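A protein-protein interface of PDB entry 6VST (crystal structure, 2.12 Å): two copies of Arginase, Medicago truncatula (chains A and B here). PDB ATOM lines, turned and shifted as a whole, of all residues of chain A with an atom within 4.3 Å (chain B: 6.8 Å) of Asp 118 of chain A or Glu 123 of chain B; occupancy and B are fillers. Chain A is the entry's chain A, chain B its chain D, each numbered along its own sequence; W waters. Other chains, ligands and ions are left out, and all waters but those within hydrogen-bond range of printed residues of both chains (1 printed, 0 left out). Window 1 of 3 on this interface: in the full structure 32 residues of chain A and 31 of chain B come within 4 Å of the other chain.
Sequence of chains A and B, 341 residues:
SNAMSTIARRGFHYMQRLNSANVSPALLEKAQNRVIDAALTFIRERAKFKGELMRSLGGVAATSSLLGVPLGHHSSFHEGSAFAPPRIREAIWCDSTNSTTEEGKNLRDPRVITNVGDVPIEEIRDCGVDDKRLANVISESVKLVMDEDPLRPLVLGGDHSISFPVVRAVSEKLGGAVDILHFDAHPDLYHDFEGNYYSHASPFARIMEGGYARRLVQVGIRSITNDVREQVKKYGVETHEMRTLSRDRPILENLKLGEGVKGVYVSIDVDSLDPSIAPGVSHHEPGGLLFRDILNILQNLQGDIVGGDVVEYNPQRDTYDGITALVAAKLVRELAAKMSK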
ATOM      1  N   PHE A  42      19.927 -25.108  -7.760  1.00  0.00           N
ATOM      2  CA  PHE A  42      20.090 -23.871  -8.514  1.00  0.00           C
ATOM      3  C   PHE A  42      20.086 -22.656  -7.588  1.00  0.00           C
ATOM      4  O   PHE A  42      20.982 -21.803  -7.660  1.00  0.00           O
ATOM      5  CB  PHE A  42      18.997 -23.730  -9.575  1.00  0.00           C
ATOM      6  CG  PHE A  42      19.171 -22.506 -10.436  1.00  0.00           C
ATOM      7  CD1 PHE A  42      20.161 -22.471 -11.415  1.00  0.00           C
ATOM      8  CD2 PHE A  42      18.390 -21.376 -10.233  1.00  0.00           C
ATOM      9  CE1 PHE A  42      20.351 -21.353 -12.191  1.00  0.00           C
ATOM     10  CE2 PHE A  42      18.571 -20.243 -11.024  1.00  0.00           C
ATOM     11  CZ  PHE A  42      19.556 -20.237 -11.997  1.00  0.00           C
ATOM     12  N   ILE A  43      19.073 -22.551  -6.719  1.00  0.00           N
ATOM     13  CA  ILE A  43      19.036 -21.424  -5.792  1.00  0.00           C
ATOM     14  C   ILE A  43      20.280 -21.413  -4.916  1.00  0.00           C
ATOM     15  O   ILE A  43      20.904 -20.361  -4.717  1.00  0.00           O
ATOM     16  CB  ILE A  43      17.756 -21.452  -4.938  1.00  0.00           C
ATOM     17  CG1 ILE A  43      16.533 -21.200  -5.814  1.00  0.00           C
ATOM     18  CG2 ILE A  43      17.832 -20.371  -3.878  1.00  0.00           C
ATOM     19  CD1 ILE A  43      16.581 -19.876  -6.522  1.00  0.00           C
ATOM     20  N   ARG A  46      23.326 -19.984  -6.621  1.00  0.00           N
ATOM     21  CA  ARG A  46      23.221 -18.543  -6.845  1.00  0.00           C
ATOM     22  C   ARG A  46      23.488 -17.780  -5.561  1.00  0.00           C
ATOM     23  O   ARG A  46      24.218 -16.782  -5.558  1.00  0.00           O
ATOM     24  CB  ARG A  46      21.838 -18.185  -7.401  1.00  0.00           C
ATOM     25  CG  ARG A  46      21.666 -18.515  -8.884  1.00  0.00           C
ATOM     26  CD  ARG A  46      22.410 -17.511  -9.770  1.00  0.00           C
ATOM     27  NE  ARG A  46      21.813 -16.190  -9.630  1.00  0.00           N
ATOM     28  CZ  ARG A  46      22.351 -15.054 -10.056  1.00  0.00           C
ATOM     29  NH1 ARG A  46      23.530 -15.039 -10.670  1.00  0.00           N
ATOM     30  NH2 ARG A  46      21.691 -13.925  -9.842  1.00  0.00           N
ATOM     31  N   GLY A  68      12.817 -14.267  -6.083  1.00  0.00           N
ATOM     32  CA  GLY A  68      11.490 -14.203  -6.672  1.00  0.00           C
ATOM     33  C   GLY A  68      10.671 -15.430  -6.298  1.00  0.00           C
ATOM     34  O   GLY A  68      11.170 -16.559  -6.289  1.00  0.00           O
ATOM     35  N   PRO A  85       7.938 -10.770 -10.512  1.00  0.00           N
ATOM     36  CA  PRO A  85       9.353 -10.614 -10.105  1.00  0.00           C
ATOM     37  C   PRO A  85      10.251 -10.113 -11.226  1.00  0.00           C
ATOM     38  O   PRO A  85      10.956  -9.116 -11.028  1.00  0.00           O
ATOM     39  CB  PRO A  85       9.741 -12.024  -9.628  1.00  0.00           C
ATOM     40  CG  PRO A  85       8.481 -12.526  -9.003  1.00  0.00           C
ATOM     41  CD  PRO A  85       7.372 -12.022  -9.959  1.00  0.00           C
ATOM     42  N   PRO A  86      10.242 -10.716 -12.427  1.00  0.00           N
ATOM     43  CA  PRO A  86      11.160 -10.211 -13.465  1.00  0.00           C
ATOM     44  C   PRO A  86      10.838  -8.790 -13.914  1.00  0.00           C
ATOM     45  O   PRO A  86      11.754  -8.048 -14.296  1.00  0.00           O
ATOM     46  CB  PRO A  86      10.988 -11.207 -14.625  1.00  0.00           C
ATOM     47  CG  PRO A  86      10.168 -12.335 -14.088  1.00  0.00           C
ATOM     48  CD  PRO A  86       9.380 -11.791 -12.956  1.00  0.00           C
ATOM     49  N   ARG A  89      12.395  -6.500 -11.222  1.00  0.00           N
ATOM     50  CA  ARG A  89      13.851  -6.416 -11.342  1.00  0.00           C
ATOM     51  C   ARG A  89      14.240  -5.536 -12.514  1.00  0.00           C
ATOM     52  O   ARG A  89      15.137  -4.695 -12.392  1.00  0.00           O
ATOM     53  CB  ARG A  89      14.481  -7.811 -11.476  1.00  0.00           C
ATOM     54  CG  ARG A  89      14.465  -8.625 -10.182  1.00  0.00           C
ATOM     55  CD  ARG A  89      15.325  -9.868 -10.303  1.00  0.00           C
ATOM     56  NE  ARG A  89      14.834 -10.714 -11.387  1.00  0.00           N
ATOM     57  CZ  ARG A  89      13.914 -11.659 -11.237  1.00  0.00           C
ATOM     58  NH1 ARG A  89      13.393 -11.882 -10.050  1.00  0.00           N
ATOM     59  NH2 ARG A  89      13.512 -12.376 -12.275  1.00  0.00           N
ATOM     60  N   VAL A 116      19.226 -12.929  -6.384  1.00  0.00           N
ATOM     61  CA  VAL A 116      19.544 -14.350  -6.259  1.00  0.00           C
ATOM     62  C   VAL A 116      18.912 -15.090  -7.433  1.00  0.00           C
ATOM     63  O   VAL A 116      19.621 -15.678  -8.253  1.00  0.00           O
ATOM     64  CB  VAL A 116      19.082 -14.931  -4.910  1.00  0.00           C
ATOM     65  CG1 VAL A 116      19.535 -16.377  -4.768  1.00  0.00           C
ATOM     66  CG2 VAL A 116      19.639 -14.105  -3.775  1.00  0.00           C
ATOM     67  N   GLY A 117      17.596 -15.031  -7.551  1.00  0.00           N
ATOM     68  CA  GLY A 117      16.894 -15.684  -8.640  1.00  0.00           C
ATOM     69  C   GLY A 117      15.461 -15.986  -8.231  1.00  0.00           C
ATOM     70  O   GLY A 117      14.996 -15.541  -7.187  1.00  0.00           O
ATOM     71  N   ASP A 118      14.777 -16.764  -9.074  1.00  0.00           N
ATOM     72  CA  ASP A 118      13.368 -17.104  -8.886  1.00  0.00           C
ATOM     73  C   ASP A 118      13.194 -18.581  -8.534  1.00  0.00           C
ATOM     74  O   ASP A 118      13.779 -19.453  -9.184  1.00  0.00           O
ATOM     75  CB  ASP A 118      12.543 -16.801 -10.149  1.00  0.00           C
ATOM     76  CG  ASP A 118      12.391 -15.300 -10.429  1.00  0.00           C
ATOM     77  OD1 ASP A 118      12.579 -14.487  -9.501  1.00  0.00           O
ATOM     78  OD2 ASP A 118      12.083 -14.939 -11.589  1.00  0.00           O
ATOM     79  N   VAL A 119      12.361 -18.858  -7.534  1.00  0.00           N
ATOM     80  CA  VAL A 119      11.909 -20.242  -7.315  1.00  0.00           C
ATOM     81  C   VAL A 119      11.095 -20.692  -8.524  1.00  0.00           C
ATOM     82  O   VAL A 119      10.157 -19.981  -8.940  1.00  0.00           O
ATOM     83  CB  VAL A 119      11.072 -20.336  -6.023  1.00  0.00           C
ATOM     84  CG1 VAL A 119      10.610 -21.772  -5.773  1.00  0.00           C
ATOM     85  CG2 VAL A 119      11.856 -19.814  -4.828  1.00  0.00           C
ATOM     86  N   PRO A 120      11.400 -21.827  -9.151  1.00  0.00           N
ATOM     87  CA  PRO A 120      10.585 -22.186 -10.339  1.00  0.00           C
ATOM     88  C   PRO A 120       9.252 -22.831  -9.955  1.00  0.00           C
ATOM     89  O   PRO A 120       9.029 -24.043 -10.044  1.00  0.00           O
ATOM     90  CB  PRO A 120      11.510 -23.130 -11.108  1.00  0.00           C
ATOM     91  CG  PRO A 120      12.345 -23.756 -10.048  1.00  0.00           C
ATOM     92  CD  PRO A 120      12.555 -22.725  -8.976  1.00  0.00           C
ATOM     93  N   VAL B  35      26.555 -22.385 -11.672  1.00  0.00           N
ATOM     94  CA  VAL B  35      25.179 -21.956 -11.951  1.00  0.00           C
ATOM     95  C   VAL B  35      24.673 -22.574 -13.254  1.00  0.00           C
ATOM     96  O   VAL B  35      23.544 -23.074 -13.324  1.00  0.00           O
ATOM     97  CB  VAL B  35      25.091 -20.420 -11.991  1.00  0.00           C
ATOM     98  CG1 VAL B  35      23.813 -19.973 -12.705  1.00  0.00           C
ATOM     99  CG2 VAL B  35      25.150 -19.860 -10.583  1.00  0.00           C
ATOM    100  N   VAL B 119      14.997 -22.003 -19.773  1.00  0.00           N
ATOM    101  CA  VAL B 119      16.413 -21.699 -19.541  1.00  0.00           C
ATOM    102  C   VAL B 119      16.502 -20.417 -18.718  1.00  0.00           C
ATOM    103  O   VAL B 119      15.861 -19.415 -19.074  1.00  0.00           O
ATOM    104  CB  VAL B 119      17.146 -21.545 -20.871  1.00  0.00           C
ATOM    105  CG1 VAL B 119      18.649 -21.374 -20.638  1.00  0.00           C
ATOM    106  CG2 VAL B 119      16.845 -22.734 -21.793  1.00  0.00           C
ATOM    107  N   PRO B 120      17.241 -20.392 -17.615  1.00  0.00           N
ATOM    108  CA  PRO B 120      17.266 -19.159 -16.786  1.00  0.00           C
ATOM    109  C   PRO B 120      18.275 -18.126 -17.295  1.00  0.00           C
ATOM    110  O   PRO B 120      19.346 -17.920 -16.741  1.00  0.00           O
ATOM    111  CB  PRO B 120      17.626 -19.696 -15.402  1.00  0.00           C
ATOM    112  CG  PRO B 120      18.475 -20.921 -15.698  1.00  0.00           C
ATOM    113  CD  PRO B 120      17.956 -21.516 -16.981  1.00  0.00           C
ATOM    114  N   ILE B 121      17.885 -17.436 -18.374  1.00  0.00           N
ATOM    115  CA  ILE B 121      18.792 -16.522 -19.071  1.00  0.00           C
ATOM    116  C   ILE B 121      19.279 -15.419 -18.137  1.00  0.00           C
ATOM    117  O   ILE B 121      20.480 -15.120 -18.081  1.00  0.00           O
ATOM    118  CB  ILE B 121      18.104 -15.943 -20.321  1.00  0.00           C
ATOM    119  CG1 ILE B 121      17.865 -17.049 -21.361  1.00  0.00           C
ATOM    120  CG2 ILE B 121      18.925 -14.816 -20.916  1.00  0.00           C
ATOM    121  CD1 ILE B 121      19.124 -17.804 -21.777  1.00  0.00           C
ATOM    122  N   GLU B 122      18.358 -14.829 -17.362  1.00  0.00           N
ATOM    123  CA  GLU B 122      18.692 -13.676 -16.526  1.00  0.00           C
ATOM    124  C   GLU B 122      19.721 -14.041 -15.465  1.00  0.00           C
ATOM    125  O   GLU B 122      20.689 -13.302 -15.244  1.00  0.00           O
ATOM    126  CB  GLU B 122      17.419 -13.108 -15.879  1.00  0.00           C
ATOM    127  CG  GLU B 122      17.638 -11.856 -15.017  1.00  0.00           C
ATOM    128  CD  GLU B 122      16.333 -11.250 -14.427  1.00  0.00           C
ATOM    129  OE1 GLU B 122      15.236 -11.848 -14.563  1.00  0.00           O
ATOM    130  OE2 GLU B 122      16.415 -10.160 -13.809  1.00  0.00           O
ATOM    131  N   GLU B 123      19.531 -15.183 -14.800  1.00  0.00           N
ATOM    132  CA  GLU B 123      20.450 -15.582 -13.744  1.00  0.00           C
ATOM    133  C   GLU B 123      21.814 -15.964 -14.299  1.00  0.00           C
ATOM    134  O   GLU B 123      22.830 -15.706 -13.647  1.00  0.00           O
ATOM    135  CB  GLU B 123      19.864 -16.736 -12.931  1.00  0.00           C
ATOM    136  CG  GLU B 123      18.678 -16.340 -12.061  1.00  0.00           C
ATOM    137  CD  GLU B 123      17.338 -16.548 -12.756  1.00  0.00           C
ATOM    138  OE1 GLU B 123      17.270 -16.374 -13.996  1.00  0.00           O
ATOM    139  OE2 GLU B 123      16.357 -16.908 -12.054  1.00  0.00           O
ATOM    140  N   ILE B 124      21.861 -16.556 -15.493  1.00  0.00           N
ATOM    141  CA  ILE B 124      23.147 -16.905 -16.098  1.00  0.00           C
ATOM    142  C   ILE B 124      23.896 -15.646 -16.539  1.00  0.00           C
ATOM    143  O   ILE B 124      25.082 -15.482 -16.237  1.00  0.00           O
ATOM    144  CB  ILE B 124      22.937 -17.896 -17.255  1.00  0.00           C
ATOM    145  CG1 ILE B 124      22.617 -19.285 -16.690  1.00  0.00           C
ATOM    146  CG2 ILE B 124      24.171 -17.968 -18.147  1.00  0.00           C
ATOM    147  CD1 ILE B 124      21.748 -20.123 -17.593  1.00  0.00           C
ATOM    148  N   ARG B 125      23.212 -14.734 -17.241  1.00  0.00           N
ATOM    149  CA  ARG B 125      23.809 -13.442 -17.593  1.00  0.00           C
ATOM    150  C   ARG B 125      24.359 -12.711 -16.375  1.00  0.00           C
ATOM    151  O   ARG B 125      25.466 -12.161 -16.421  1.00  0.00           O
ATOM    152  CB  ARG B 125      22.780 -12.548 -18.278  1.00  0.00           C
ATOM    153  CG  ARG B 125      22.523 -12.867 -19.709  1.00  0.00           C
ATOM    154  CD  ARG B 125      21.578 -11.837 -20.285  1.00  0.00           C
ATOM    155  NE  ARG B 125      22.240 -10.583 -20.627  1.00  0.00           N
ATOM    156  CZ  ARG B 125      21.614  -9.411 -20.674  1.00  0.00           C
ATOM    157  NH1 ARG B 125      22.270  -8.309 -21.009  1.00  0.00           N
ATOM    158  NH2 ARG B 125      20.325  -9.339 -20.378  1.00  0.00           N
ATOM    159  N   ASP B 126      23.595 -12.685 -15.274  1.00  0.00           N
ATOM    160  CA  ASP B 126      24.053 -12.053 -14.043  1.00  0.00           C
ATOM    161  C   ASP B 126      25.342 -12.674 -13.499  1.00  0.00           C
ATOM    162  O   ASP B 126      25.931 -12.125 -12.559  1.00  0.00           O
ATOM    163  CB  ASP B 126      22.940 -12.115 -12.982  1.00  0.00           C
ATOM    164  CG  ASP B 126      23.221 -11.219 -11.771  1.00  0.00           C
ATOM    165  OD1 ASP B 126      23.600 -10.046 -11.967  1.00  0.00           O
ATOM    166  OD2 ASP B 126      23.062 -11.678 -10.617  1.00  0.00           O
ATOM    167  N   CYS B 127      25.799 -13.797 -14.051  1.00  0.00           N
ATOM    168  CA  CYS B 127      27.104 -14.331 -13.686  1.00  0.00           C
ATOM    169  C   CYS B 127      28.225 -13.816 -14.576  1.00  0.00           C
ATOM    170  O   CYS B 127      29.376 -14.238 -14.402  1.00  0.00           O
ATOM    171  CB  CYS B 127      27.085 -15.859 -13.735  1.00  0.00           C
ATOM    172  SG  CYS B 127      26.018 -16.626 -12.511  1.00  0.00           S
ATOM    173  N   GLY B 128      27.925 -12.933 -15.530  1.00  0.00           N
ATOM    174  CA  GLY B 128      28.943 -12.427 -16.429  1.00  0.00           C
ATOM    175  C   GLY B 128      29.217 -13.305 -17.624  1.00  0.00           C
ATOM    176  O   GLY B 128      30.207 -13.082 -18.323  1.00  0.00           O
HETATM  177  O   HOH W   1      14.152  -8.758 -15.269  1.00  0.00           O
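NH1 of Arg 46 of chain A sits at hydrogen-bond distance from O of Glu 123 of chain B. NH2 of Arg 46 of chain A lies within salt-bridge range of OD2 of Asp 126 of chain B, 2.7 Å away. The guanidinium group (NH1) of Arg 46 of chain A sits at hydrogen-bond distance from the side-chain sulfur (SG) of Cys 127 of chain B, 3.5 Å away. NH2 of Arg 89 of chain A lies within salt-bridge range of OE1 of Glu 122 of chain B (2.9 Å). OE2 of Glu 123 of chain B lies within hydrogen-bond range of N of Asp 118 of chain A, at 3.4 Å.
O of Val 116 of chain A sits at hydrogen-bond distance from NE of Arg 46 of chain A. N of Gly 68 of chain A lies within hydrogen-bond range of O of Gly 117 of chain A, 2.8 Å away. The backbone NH (N) of Gly 68 of chain A lies close to the side-chain carboxylate (OD1) of Asp 118 of chain A, at 3.4 Å. The side-chain carboxylate (OD1) of Asp 118 of chain A lies within salt-bridge range of the guanidinium group (NH1) of Arg 89 of chain A, 2.8 Å away. The backbone carbonyl oxygen (O) of Glu 123 of chain B is in hydrogen-bond range of the side-chain sulfur (SG) of Cys 127 of chain B (3.5 Å).
Phe 42 of chain A touches Val 35 of chain B (CE1 to CG1, 3.8 Å). Phe 42 of chain A touches Pro 120 of chain B. CZ of Phe 42 of chain A touches CB of Glu 123 of chain B, 3.6 Å away. CG2 of Val 35 of chain B touches CD of Arg 46 of chain A, 3.7 Å away. Glu 123 of chain B touches Val 116 of chain A. OE2 of Glu 123 of chain B touches CA of Gly 117 of chain A, at 3.7 Å.
Of the printed residues of chain B, Phe 42 of chain A touches Val 35 (3.8 Å), Pro 120 (3.9 Å) and Glu 123 (3.6 Å). Gly 68 of chain A touches none of the printed residues of chain B. Of the printed residues of chain B, Val 116 of chain A touches Glu 123 (3.98 Å). Of chain B, only Glu 123 (3.4 Å) comes within 4 Å of Asp 118 of chain A. Of the printed residues of chain A, Val 35 of chain B touches Phe 42 (3.8 Å) and Arg 46 (3.7 Å). Printed residues of chain A within 4 Å of Pro 120 of chain B: Phe 42. Ile 121 of chain B touches none of the printed residues of chain A. Glu 123 of chain B touches just these residues of chain A: Phe 42, Arg 46, Val 116, Gly 117 and Asp 118. Of the printed residues of chain A, Cys 127 of chain B touches Arg 46. The nearest residue of chain B that does not touch Asp 118 of chain A is Glu 122 of chain B (5.3 Å). The nearest printed residue of chain A that does not touch Glu 123 of chain B is Arg 89 of chain A (5.4 Å).
Hydrophobic or aromatic side chains of chain A within 4 Å of the printed part of chain B: Phe 42. Hydrophobic or aromatic side chains of chain B within 4 Å of the printed part of chain A: Val 35 and Pro 120. Among the printed residues, Asp or Glu carboxylates within 4 Å of a Lys or Arg side-chain nitrogen of the other chain: Arg 46 of chain A with Asp 126 of chain B (2.7 Å) and Arg 89 of chain A with Glu 122 of chain B (2.9 Å).
2 positions are printed for both chains. Of the 11 pairs that touch across the chains among the printed residues, none has its exchanged pair printed and touching as well.
Water W1 bridges O of Pro 86 of chain A (2.7 Å) and OE2 of Glu 122 of chain B (3.0 Å).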
